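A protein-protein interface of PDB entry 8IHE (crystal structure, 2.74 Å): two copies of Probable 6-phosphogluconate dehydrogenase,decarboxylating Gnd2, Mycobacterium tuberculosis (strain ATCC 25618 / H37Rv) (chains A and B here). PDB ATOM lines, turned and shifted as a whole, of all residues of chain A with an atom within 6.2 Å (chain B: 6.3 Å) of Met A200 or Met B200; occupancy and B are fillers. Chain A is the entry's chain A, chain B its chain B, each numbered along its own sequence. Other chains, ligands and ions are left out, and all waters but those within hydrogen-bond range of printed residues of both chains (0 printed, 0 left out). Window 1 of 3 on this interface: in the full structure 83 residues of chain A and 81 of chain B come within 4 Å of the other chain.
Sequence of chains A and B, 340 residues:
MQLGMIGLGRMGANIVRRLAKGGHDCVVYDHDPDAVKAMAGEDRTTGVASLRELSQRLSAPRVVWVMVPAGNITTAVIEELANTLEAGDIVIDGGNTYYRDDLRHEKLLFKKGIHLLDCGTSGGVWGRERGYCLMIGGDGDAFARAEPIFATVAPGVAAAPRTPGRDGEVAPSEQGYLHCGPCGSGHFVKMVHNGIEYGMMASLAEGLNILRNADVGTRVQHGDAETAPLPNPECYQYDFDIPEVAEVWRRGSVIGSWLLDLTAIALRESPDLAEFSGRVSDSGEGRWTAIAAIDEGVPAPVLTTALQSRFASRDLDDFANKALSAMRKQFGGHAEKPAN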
ATOM      1  N   GLY A 195      16.957  25.360 -28.479  1.00  0.00           N
ATOM      2  CA  GLY A 195      17.160  25.785 -27.083  1.00  0.00           C
ATOM      3  C   GLY A 195      16.748  24.677 -26.138  1.00  0.00           C
ATOM      4  O   GLY A 195      17.598  24.237 -25.277  1.00  0.00           O
ATOM      5  N   ILE A 196      15.528  24.174 -26.328  1.00  0.00           N
ATOM      6  CA  ILE A 196      14.970  23.088 -25.470  1.00  0.00           C
ATOM      7  C   ILE A 196      15.856  21.840 -25.571  1.00  0.00           C
ATOM      8  O   ILE A 196      15.984  21.149 -24.577  1.00  0.00           O
ATOM      9  CB  ILE A 196      13.515  22.797 -25.852  1.00  0.00           C
ATOM     10  CG1 ILE A 196      12.668  24.063 -25.722  1.00  0.00           C
ATOM     11  CG2 ILE A 196      12.988  21.656 -24.994  1.00  0.00           C
ATOM     12  CD1 ILE A 196      11.210  23.935 -26.111  1.00  0.00           C
ATOM     13  N   GLU A 197      16.370  21.536 -26.764  1.00  0.00           N
ATOM     14  CA  GLU A 197      17.283  20.410 -27.035  1.00  0.00           C
ATOM     15  C   GLU A 197      18.483  20.556 -26.104  1.00  0.00           C
ATOM     16  O   GLU A 197      18.761  19.620 -25.347  1.00  0.00           O
ATOM     17  CB  GLU A 197      17.657  20.451 -28.509  1.00  0.00           C
ATOM     18  CG  GLU A 197      18.525  19.293 -28.974  1.00  0.00           C
ATOM     19  CD  GLU A 197      19.132  19.499 -30.354  1.00  0.00           C
ATOM     20  OE1 GLU A 197      20.274  20.079 -30.424  1.00  0.00           O
ATOM     21  OE2 GLU A 197      18.464  19.108 -31.366  1.00  0.00           O
ATOM     22  N   TYR A 198      19.113  21.729 -26.090  1.00  0.00           N
ATOM     23  CA  TYR A 198      20.308  22.029 -25.252  1.00  0.00           C
ATOM     24  C   TYR A 198      19.935  21.767 -23.784  1.00  0.00           C
ATOM     25  O   TYR A 198      20.735  21.236 -23.006  1.00  0.00           O
ATOM     26  CB  TYR A 198      20.826  23.458 -25.480  1.00  0.00           C
ATOM     27  CG  TYR A 198      21.517  23.744 -26.796  1.00  0.00           C
ATOM     28  CD1 TYR A 198      21.473  22.860 -27.855  1.00  0.00           C
ATOM     29  CD2 TYR A 198      22.177  24.949 -26.998  1.00  0.00           C
ATOM     30  CE1 TYR A 198      22.101  23.144 -29.057  1.00  0.00           C
ATOM     31  CE2 TYR A 198      22.802  25.256 -28.191  1.00  0.00           C
ATOM     32  CZ  TYR A 198      22.772  24.343 -29.229  1.00  0.00           C
ATOM     33  OH  TYR A 198      23.362  24.616 -30.432  1.00  0.00           O
ATOM     34  N   GLY A 199      18.708  22.102 -23.435  1.00  0.00           N
ATOM     35  CA  GLY A 199      18.234  22.074 -22.041  1.00  0.00           C
ATOM     36  C   GLY A 199      18.005  20.663 -21.580  1.00  0.00           C
ATOM     37  O   GLY A 199      18.302  20.347 -20.427  1.00  0.00           O
ATOM     38  N   MET A 200      17.472  19.848 -22.459  1.00  0.00           N
ATOM     39  CA  MET A 200      17.216  18.441 -22.141  1.00  0.00           C
ATOM     40  C   MET A 200      18.545  17.678 -22.136  1.00  0.00           C
ATOM     41  O   MET A 200      18.752  16.867 -21.198  1.00  0.00           O
ATOM     42  CB  MET A 200      16.242  17.843 -23.147  1.00  0.00           C
ATOM     43  CG  MET A 200      14.857  18.429 -23.059  1.00  0.00           C
ATOM     44  SD  MET A 200      13.771  17.921 -24.425  1.00  0.00           S
ATOM     45  CE  MET A 200      13.662  16.168 -24.075  1.00  0.00           C
ATOM     46  N   MET A 201      19.446  17.951 -23.082  1.00  0.00           N
ATOM     47  CA  MET A 201      20.796  17.303 -23.107  1.00  0.00           C
ATOM     48  C   MET A 201      21.585  17.621 -21.819  1.00  0.00           C
ATOM     49  O   MET A 201      22.071  16.661 -21.205  1.00  0.00           O
ATOM     50  CB  MET A 201      21.590  17.736 -24.337  1.00  0.00           C
ATOM     51  CG  MET A 201      20.927  17.241 -25.599  1.00  0.00           C
ATOM     52  SD  MET A 201      21.660  17.885 -27.086  1.00  0.00           S
ATOM     53  CE  MET A 201      23.346  17.328 -26.833  1.00  0.00           C
ATOM     54  N   ALA A 202      21.652  18.891 -21.394  1.00  0.00           N
ATOM     55  CA  ALA A 202      22.366  19.327 -20.165  1.00  0.00           C
ATOM     56  C   ALA A 202      21.808  18.587 -18.934  1.00  0.00           C
ATOM     57  O   ALA A 202      22.582  18.246 -17.996  1.00  0.00           O
ATOM     58  CB  ALA A 202      22.241  20.828 -19.967  1.00  0.00           C
ATOM     59  N   SER A 203      20.498  18.392 -18.917  1.00  0.00           N
ATOM     60  CA  SER A 203      19.770  17.865 -17.755  1.00  0.00           C
ATOM     61  C   SER A 203      20.155  16.399 -17.613  1.00  0.00           C
ATOM     62  O   SER A 203      20.591  16.012 -16.500  1.00  0.00           O
ATOM     63  CB  SER A 203      18.285  18.097 -17.905  1.00  0.00           C
ATOM     64  OG  SER A 203      17.972  19.485 -17.811  1.00  0.00           O
ATOM     65  N   LEU A 204      20.118  15.640 -18.721  1.00  0.00           N
ATOM     66  CA  LEU A 204      20.674  14.248 -18.785  1.00  0.00           C
ATOM     67  C   LEU A 204      22.158  14.201 -18.396  1.00  0.00           C
ATOM     68  O   LEU A 204      22.482  13.348 -17.558  1.00  0.00           O
ATOM     69  CB  LEU A 204      20.462  13.650 -20.168  1.00  0.00           C
ATOM     70  CG  LEU A 204      19.171  12.852 -20.305  1.00  0.00           C
ATOM     71  CD1 LEU A 204      18.919  12.448 -21.753  1.00  0.00           C
ATOM     72  CD2 LEU A 204      19.245  11.623 -19.447  1.00  0.00           C
ATOM     73  N   ALA A 205      22.992  15.101 -18.909  1.00  0.00           N
ATOM     74  CA  ALA A 205      24.456  15.077 -18.707  1.00  0.00           C
ATOM     75  C   ALA A 205      24.799  15.369 -17.246  1.00  0.00           C
ATOM     76  O   ALA A 205      25.621  14.642 -16.675  1.00  0.00           O
ATOM     77  CB  ALA A 205      25.140  16.063 -19.621  1.00  0.00           C
ATOM     78  N   VAL A 254       9.465   9.001 -16.020  1.00  0.00           N
ATOM     79  CA  VAL A 254       8.939  10.346 -16.420  1.00  0.00           C
ATOM     80  C   VAL A 254       9.853  10.995 -17.482  1.00  0.00           C
ATOM     81  O   VAL A 254       9.390  11.885 -18.244  1.00  0.00           O
ATOM     82  CB  VAL A 254       8.804  11.256 -15.182  1.00  0.00           C
ATOM     83  CG1 VAL A 254       7.971  12.493 -15.478  1.00  0.00           C
ATOM     84  CG2 VAL A 254       8.227  10.517 -14.000  1.00  0.00           C
ATOM     85  N   ILE A 255      11.124  10.586 -17.549  1.00  0.00           N
ATOM     86  CA  ILE A 255      12.161  11.227 -18.407  1.00  0.00           C
ATOM     87  C   ILE A 255      12.378  10.414 -19.683  1.00  0.00           C
ATOM     88  O   ILE A 255      13.318  10.699 -20.431  1.00  0.00           O
ATOM     89  CB  ILE A 255      13.461  11.429 -17.616  1.00  0.00           C
ATOM     90  CG1 ILE A 255      14.299  10.153 -17.538  1.00  0.00           C
ATOM     91  CG2 ILE A 255      13.146  11.993 -16.237  1.00  0.00           C
ATOM     92  CD1 ILE A 255      15.431  10.231 -16.527  1.00  0.00           C
ATOM     93  N   GLY A 256      11.530   9.443 -19.947  1.00  0.00           N
ATOM     94  CA  GLY A 256      11.432   8.851 -21.288  1.00  0.00           C
ATOM     95  C   GLY A 256      11.445   9.965 -22.319  1.00  0.00           C
ATOM     96  O   GLY A 256      10.655  10.923 -22.142  1.00  0.00           O
ATOM     97  N   SER A 257      12.342   9.838 -23.311  1.00  0.00           N
ATOM     98  CA  SER A 257      12.626  10.767 -24.436  1.00  0.00           C
ATOM     99  C   SER A 257      13.564  10.096 -25.455  1.00  0.00           C
ATOM    100  O   SER A 257      14.356   9.257 -25.060  1.00  0.00           O
ATOM    101  CB  SER A 257      13.272  12.005 -23.886  1.00  0.00           C
ATOM    102  OG  SER A 257      14.615  11.738 -23.469  1.00  0.00           O
ATOM    103  N   LEU A 259      16.324  11.524 -26.641  1.00  0.00           N
ATOM    104  CA  LEU A 259      17.686  11.822 -26.130  1.00  0.00           C
ATOM    105  C   LEU A 259      18.109  10.798 -25.082  1.00  0.00           C
ATOM    106  O   LEU A 259      19.299  10.519 -25.080  1.00  0.00           O
ATOM    107  CB  LEU A 259      17.727  13.234 -25.539  1.00  0.00           C
ATOM    108  CG  LEU A 259      17.484  14.360 -26.542  1.00  0.00           C
ATOM    109  CD1 LEU A 259      17.290  15.673 -25.798  1.00  0.00           C
ATOM    110  CD2 LEU A 259      18.610  14.436 -27.577  1.00  0.00           C
ATOM    111  N   VAL A 302      17.431  27.946 -17.177  1.00  0.00           N
ATOM    112  CA  VAL A 302      17.738  26.520 -17.486  1.00  0.00           C
ATOM    113  C   VAL A 302      18.275  26.380 -18.909  1.00  0.00           C
ATOM    114  O   VAL A 302      19.418  25.813 -19.056  1.00  0.00           O
ATOM    115  CB  VAL A 302      16.554  25.598 -17.245  1.00  0.00           C
ATOM    116  CG1 VAL A 302      16.906  24.148 -17.532  1.00  0.00           C
ATOM    117  CG2 VAL A 302      16.028  25.740 -15.820  1.00  0.00           C
ATOM    118  N   LEU A 303      17.580  26.917 -19.913  1.00  0.00           N
ATOM    119  CA  LEU A 303      18.090  26.969 -21.323  1.00  0.00           C
ATOM    120  C   LEU A 303      19.399  27.777 -21.384  1.00  0.00           C
ATOM    121  O   LEU A 303      20.354  27.342 -22.095  1.00  0.00           O
ATOM    122  CB  LEU A 303      17.068  27.599 -22.258  1.00  0.00           C
ATOM    123  CG  LEU A 303      15.704  26.918 -22.316  1.00  0.00           C
ATOM    124  CD1 LEU A 303      14.876  27.531 -23.428  1.00  0.00           C
ATOM    125  CD2 LEU A 303      15.814  25.403 -22.494  1.00  0.00           C
ATOM    126  N   ALA A 306      22.409  25.966 -19.843  1.00  0.00           N
ATOM    127  CA  ALA A 306      22.756  24.820 -20.716  1.00  0.00           C
ATOM    128  C   ALA A 306      23.674  25.333 -21.809  1.00  0.00           C
ATOM    129  O   ALA A 306      24.737  24.752 -22.005  1.00  0.00           O
ATOM    130  CB  ALA A 306      21.541  24.187 -21.343  1.00  0.00           C
ATOM    131  N   GLY B 195      15.670  15.104 -10.261  1.00  0.00           N
ATOM    132  CA  GLY B 195      16.580  16.186 -10.705  1.00  0.00           C
ATOM    133  C   GLY B 195      16.552  16.332 -12.230  1.00  0.00           C
ATOM    134  O   GLY B 195      16.231  17.439 -12.727  1.00  0.00           O
ATOM    135  N   ILE B 196      16.784  15.244 -12.961  1.00  0.00           N
ATOM    136  CA  ILE B 196      16.746  15.290 -14.443  1.00  0.00           C
ATOM    137  C   ILE B 196      15.315  15.701 -14.848  1.00  0.00           C
ATOM    138  O   ILE B 196      15.155  16.559 -15.765  1.00  0.00           O
ATOM    139  CB  ILE B 196      17.227  13.944 -15.042  1.00  0.00           C
ATOM    140  CG1 ILE B 196      18.725  13.721 -14.872  1.00  0.00           C
ATOM    141  CG2 ILE B 196      16.852  13.792 -16.505  1.00  0.00           C
ATOM    142  CD1 ILE B 196      19.134  12.255 -15.010  1.00  0.00           C
ATOM    143  N   GLU B 197      14.296  15.095 -14.235  1.00  0.00           N
ATOM    144  CA  GLU B 197      12.882  15.382 -14.579  1.00  0.00           C
ATOM    145  C   GLU B 197      12.608  16.887 -14.394  1.00  0.00           C
ATOM    146  O   GLU B 197      11.876  17.480 -15.173  1.00  0.00           O
ATOM    147  CB  GLU B 197      11.993  14.493 -13.723  1.00  0.00           C
ATOM    148  CG  GLU B 197      10.508  14.800 -13.819  1.00  0.00           C
ATOM    149  CD  GLU B 197       9.750  14.340 -12.576  1.00  0.00           C
ATOM    150  OE1 GLU B 197       9.798  15.094 -11.576  1.00  0.00           O
ATOM    151  OE2 GLU B 197       9.177  13.193 -12.579  1.00  0.00           O
ATOM    152  N   TYR B 198      13.187  17.523 -13.399  1.00  0.00           N
ATOM    153  CA  TYR B 198      12.936  18.961 -13.174  1.00  0.00           C
ATOM    154  C   TYR B 198      13.525  19.729 -14.361  1.00  0.00           C
ATOM    155  O   TYR B 198      12.911  20.712 -14.838  1.00  0.00           O
ATOM    156  CB  TYR B 198      13.570  19.432 -11.866  1.00  0.00           C
ATOM    157  CG  TYR B 198      12.885  19.072 -10.570  1.00  0.00           C
ATOM    158  CD1 TYR B 198      11.830  18.175 -10.478  1.00  0.00           C
ATOM    159  CD2 TYR B 198      13.329  19.679  -9.397  1.00  0.00           C
ATOM    160  CE1 TYR B 198      11.261  17.871  -9.248  1.00  0.00           C
ATOM    161  CE2 TYR B 198      12.755  19.402  -8.173  1.00  0.00           C
ATOM    162  CZ  TYR B 198      11.742  18.471  -8.095  1.00  0.00           C
ATOM    163  OH  TYR B 198      11.277  18.231  -6.845  1.00  0.00           O
ATOM    164  N   GLY B 199      14.725  19.326 -14.786  1.00  0.00           N
ATOM    165  CA  GLY B 199      15.481  20.038 -15.832  1.00  0.00           C
ATOM    166  C   GLY B 199      14.812  19.884 -17.191  1.00  0.00           C
ATOM    167  O   GLY B 199      14.781  20.879 -17.983  1.00  0.00           O
ATOM    168  N   MET B 200      14.292  18.694 -17.478  1.00  0.00           N
ATOM    169  CA  MET B 200      13.576  18.471 -18.751  1.00  0.00           C
ATOM    170  C   MET B 200      12.272  19.302 -18.781  1.00  0.00           C
ATOM    171  O   MET B 200      12.087  20.068 -19.744  1.00  0.00           O
ATOM    172  CB  MET B 200      13.344  16.976 -18.939  1.00  0.00           C
ATOM    173  CG  MET B 200      14.644  16.239 -19.319  1.00  0.00           C
ATOM    174  SD  MET B 200      14.343  14.476 -19.442  1.00  0.00           S
ATOM    175  CE  MET B 200      13.298  14.475 -20.894  1.00  0.00           C
ATOM    176  N   MET B 201      11.447  19.241 -17.728  1.00  0.00           N
ATOM    177  CA  MET B 201      10.214  20.061 -17.537  1.00  0.00           C
ATOM    178  C   MET B 201      10.515  21.545 -17.776  1.00  0.00           C
ATOM    179  O   MET B 201       9.907  22.145 -18.685  1.00  0.00           O
ATOM    180  CB  MET B 201       9.691  19.915 -16.106  1.00  0.00           C
ATOM    181  CG  MET B 201       9.010  18.570 -15.803  1.00  0.00           C
ATOM    182  SD  MET B 201       8.809  18.271 -14.027  1.00  0.00           S
ATOM    183  CE  MET B 201       7.376  19.280 -13.663  1.00  0.00           C
ATOM    184  N   ALA B 202      11.380  22.131 -16.951  1.00  0.00           N
ATOM    185  CA  ALA B 202      11.831  23.522 -17.079  1.00  0.00           C
ATOM    186  C   ALA B 202      12.325  23.819 -18.497  1.00  0.00           C
ATOM    187  O   ALA B 202      12.168  24.981 -18.922  1.00  0.00           O
ATOM    188  CB  ALA B 202      12.949  23.767 -16.105  1.00  0.00           C
ATOM    189  N   SER B 203      12.992  22.876 -19.179  1.00  0.00           N
ATOM    190  CA  SER B 203      13.579  23.191 -20.505  1.00  0.00           C
ATOM    191  C   SER B 203      12.440  23.538 -21.476  1.00  0.00           C
ATOM    192  O   SER B 203      12.519  24.555 -22.147  1.00  0.00           O
ATOM    193  CB  SER B 203      14.479  22.082 -21.013  1.00  0.00           C
ATOM    194  OG  SER B 203      15.729  22.065 -20.327  1.00  0.00           O
ATOM    195  N   LEU B 204      11.383  22.738 -21.453  1.00  0.00           N
ATOM    196  CA  LEU B 204      10.118  22.833 -22.234  1.00  0.00           C
ATOM    197  C   LEU B 204       9.288  24.035 -21.770  1.00  0.00           C
ATOM    198  O   LEU B 204       8.801  24.800 -22.637  1.00  0.00           O
ATOM    199  CB  LEU B 204       9.345  21.549 -21.942  1.00  0.00           C
ATOM    200  CG  LEU B 204       8.676  20.863 -23.109  1.00  0.00           C
ATOM    201  CD1 LEU B 204       7.513  20.019 -22.585  1.00  0.00           C
ATOM    202  CD2 LEU B 204       8.184  21.864 -24.147  1.00  0.00           C
ATOM    203  N   ALA B 205       9.132  24.191 -20.450  1.00  0.00           N
ATOM    204  CA  ALA B 205       8.327  25.257 -19.833  1.00  0.00           C
ATOM    205  C   ALA B 205       8.905  26.601 -20.283  1.00  0.00           C
ATOM    206  O   ALA B 205       8.152  27.406 -20.847  1.00  0.00           O
ATOM    207  CB  ALA B 205       8.305  25.089 -18.324  1.00  0.00           C
ATOM    208  N   VAL B 254      13.873  16.287 -32.366  1.00  0.00           N
ATOM    209  CA  VAL B 254      14.889  15.838 -31.371  1.00  0.00           C
ATOM    210  C   VAL B 254      14.277  15.715 -29.960  1.00  0.00           C
ATOM    211  O   VAL B 254      14.708  14.789 -29.217  1.00  0.00           O
ATOM    212  CB  VAL B 254      16.092  16.782 -31.421  1.00  0.00           C
ATOM    213  CG1 VAL B 254      17.245  16.240 -30.587  1.00  0.00           C
ATOM    214  CG2 VAL B 254      16.485  17.013 -32.877  1.00  0.00           C
ATOM    215  N   ILE B 255      13.264  16.543 -29.634  1.00  0.00           N
ATOM    216  CA  ILE B 255      12.839  16.834 -28.231  1.00  0.00           C
ATOM    217  C   ILE B 255      11.618  16.011 -27.845  1.00  0.00           C
ATOM    218  O   ILE B 255      11.016  16.334 -26.812  1.00  0.00           O
ATOM    219  CB  ILE B 255      12.582  18.333 -27.993  1.00  0.00           C
ATOM    220  CG1 ILE B 255      11.372  18.831 -28.770  1.00  0.00           C
ATOM    221  CG2 ILE B 255      13.829  19.181 -28.258  1.00  0.00           C
ATOM    222  CD1 ILE B 255      10.823  20.105 -28.229  1.00  0.00           C
ATOM    223  N   GLY B 256      11.272  14.986 -28.626  1.00  0.00           N
ATOM    224  CA  GLY B 256      10.188  14.045 -28.279  1.00  0.00           C
ATOM    225  C   GLY B 256      10.440  13.458 -26.907  1.00  0.00           C
ATOM    226  O   GLY B 256      11.616  13.233 -26.575  1.00  0.00           O
ATOM    227  N   SER B 257       9.390  13.297 -26.108  1.00  0.00           N
ATOM    228  CA  SER B 257       9.488  12.892 -24.683  1.00  0.00           C
ATOM    229  C   SER B 257       8.089  12.686 -24.114  1.00  0.00           C
ATOM    230  O   SER B 257       7.141  13.350 -24.610  1.00  0.00           O
ATOM    231  CB  SER B 257      10.212  13.914 -23.870  1.00  0.00           C
ATOM    232  OG  SER B 257       9.431  15.102 -23.753  1.00  0.00           O
ATOM    233  N   LEU B 259       7.068  13.845 -21.314  1.00  0.00           N
ATOM    234  CA  LEU B 259       6.679  15.170 -20.751  1.00  0.00           C
ATOM    235  C   LEU B 259       6.126  16.054 -21.864  1.00  0.00           C
ATOM    236  O   LEU B 259       5.149  16.783 -21.580  1.00  0.00           O
ATOM    237  CB  LEU B 259       7.865  15.876 -20.100  1.00  0.00           C
ATOM    238  CG  LEU B 259       8.313  15.350 -18.743  1.00  0.00           C
ATOM    239  CD1 LEU B 259       9.579  16.062 -18.315  1.00  0.00           C
ATOM    240  CD2 LEU B 259       7.222  15.525 -17.716  1.00  0.00           C
ATOM    241  N   VAL B 302      22.084  23.732 -14.635  1.00  0.00           N
ATOM    242  CA  VAL B 302      20.822  23.525 -15.386  1.00  0.00           C
ATOM    243  C   VAL B 302      19.810  22.824 -14.465  1.00  0.00           C
ATOM    244  O   VAL B 302      18.637  23.295 -14.392  1.00  0.00           O
ATOM    245  CB  VAL B 302      21.085  22.770 -16.690  1.00  0.00           C
ATOM    246  CG1 VAL B 302      19.796  22.434 -17.439  1.00  0.00           C
ATOM    247  CG2 VAL B 302      22.036  23.529 -17.596  1.00  0.00           C
ATOM    248  N   LEU B 303      20.190  21.752 -13.771  1.00  0.00           N
ATOM    249  CA  LEU B 303      19.262  21.107 -12.807  1.00  0.00           C
ATOM    250  C   LEU B 303      18.956  22.114 -11.674  1.00  0.00           C
ATOM    251  O   LEU B 303      17.794  22.458 -11.475  1.00  0.00           O
ATOM    252  CB  LEU B 303      19.872  19.818 -12.267  1.00  0.00           C
ATOM    253  CG  LEU B 303      20.081  18.682 -13.262  1.00  0.00           C
ATOM    254  CD1 LEU B 303      20.024  17.329 -12.571  1.00  0.00           C
ATOM    255  CD2 LEU B 303      19.052  18.705 -14.370  1.00  0.00           C
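Glu A197 touches Val B254 (OE2 to CG1, 3.2 Å). Glu A197 touches Ile B255. Val A254 touches Glu B197 (CG2 to OE2, 3.2 Å). Val A254 touches Leu B259. Ser A257 touches Met B200. Ser A257 touches Gly B256. Ala B202 touches Val A302 (CB to CG2, 3.7 Å). OG of Ser B203 touches CG1 of Val A302, 3.7 Å away. Val A302 touches Val B302 (CG1 to CG1, 3.4 Å). Ser B203 touches Leu A303.
Met A200 touches just these residues of chain B: Met B200 (3.6 Å), Ser B203 (3.5 Å) and Ile B255 (3.8 Å). Printed residues of chain A within 4 Å of Met B200: Met A200, Ser A203, Ile A255 and Ser A257. Of the printed residues of chain A, Ala B202 touches Val A302. Printed residues of chain B within 4 Å of Val A254: Glu B197 (3.2 Å) and Leu B259 (3.7 Å). Printed residues of chain B within 4 Å of Ser A203: Ile B196, Gly B199, Met B200, Val B302 and Leu B303. Of the printed residues of chain A, Leu B259 touches Val A254. Ala B205 touches none of the printed residues of chain A. Ala A205 touches none of the printed residues of chain B. The nearest printed residue of chain B that does not touch Leu A303 is Ala B202 (5.1 Å).
The side-chain hydroxyl of Ser A203 sits at hydrogen-bond distance from the backbone carbonyl oxygen of Gly A199, at 2.8 Å. The backbone carbonyl oxygen of Ile A255 sits at hydrogen-bond distance from the side-chain hydroxyl of Ser A257. The side-chain hydroxyl of Ser B203 is in hydrogen-bond range of the backbone carbonyl oxygen of Gly B199, 2.8 Å away.
Printed residues of chain B that touch a printed residue of chain A: Ile B196, Glu B197, Gly B199, Met B200, Ala B202, Ser B203, Val B254, Ile B255, Gly B256, Ser B257, Leu B259, Val B302 and Leu B303. Hydrophobic or aromatic side chains of chain B within 4 Å of the printed part of chain A: Ile B196, Met B200, Ala B202, Val B254, Ile B255, Leu B259, Val B302 and Leu B303. Hydrophobic or aromatic side chains of chain A within 4 Å of the printed part of chain B: Ile A196, Met A200, Ala A202, Val A254, Ile A255, Leu A259, Val A302, Leu A303 and Ala A306. Among the printed residues, no Asp or Glu carboxylate lies within 4 Å of a Lys or Arg side-chain nitrogen of the other chain.
Glu A197 touches Ile B255, and with the chains exchanged Ile A255 touches Glu B197. Gly A199 touches Val B302, and with the chains exchanged Val A302 touches Gly B199. Ser A203 touches Leu B303, and with the chains exchanged Leu A303 touches Ser B203. Val A254 touches Leu B259, and with the chains exchanged Leu A259 touches Val B254. Positions printed for both chains: 195, 196, 197, 198, 199, 200, 201, 202, 203, 204, 205, 254, 255, 256, 257, 259, 302 and 303.
OG of Ser B203 sits close to O of Gly A199 (3.1 Å). OG of Ser A203 lies close to O of Gly B199, at 3.5 Å.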
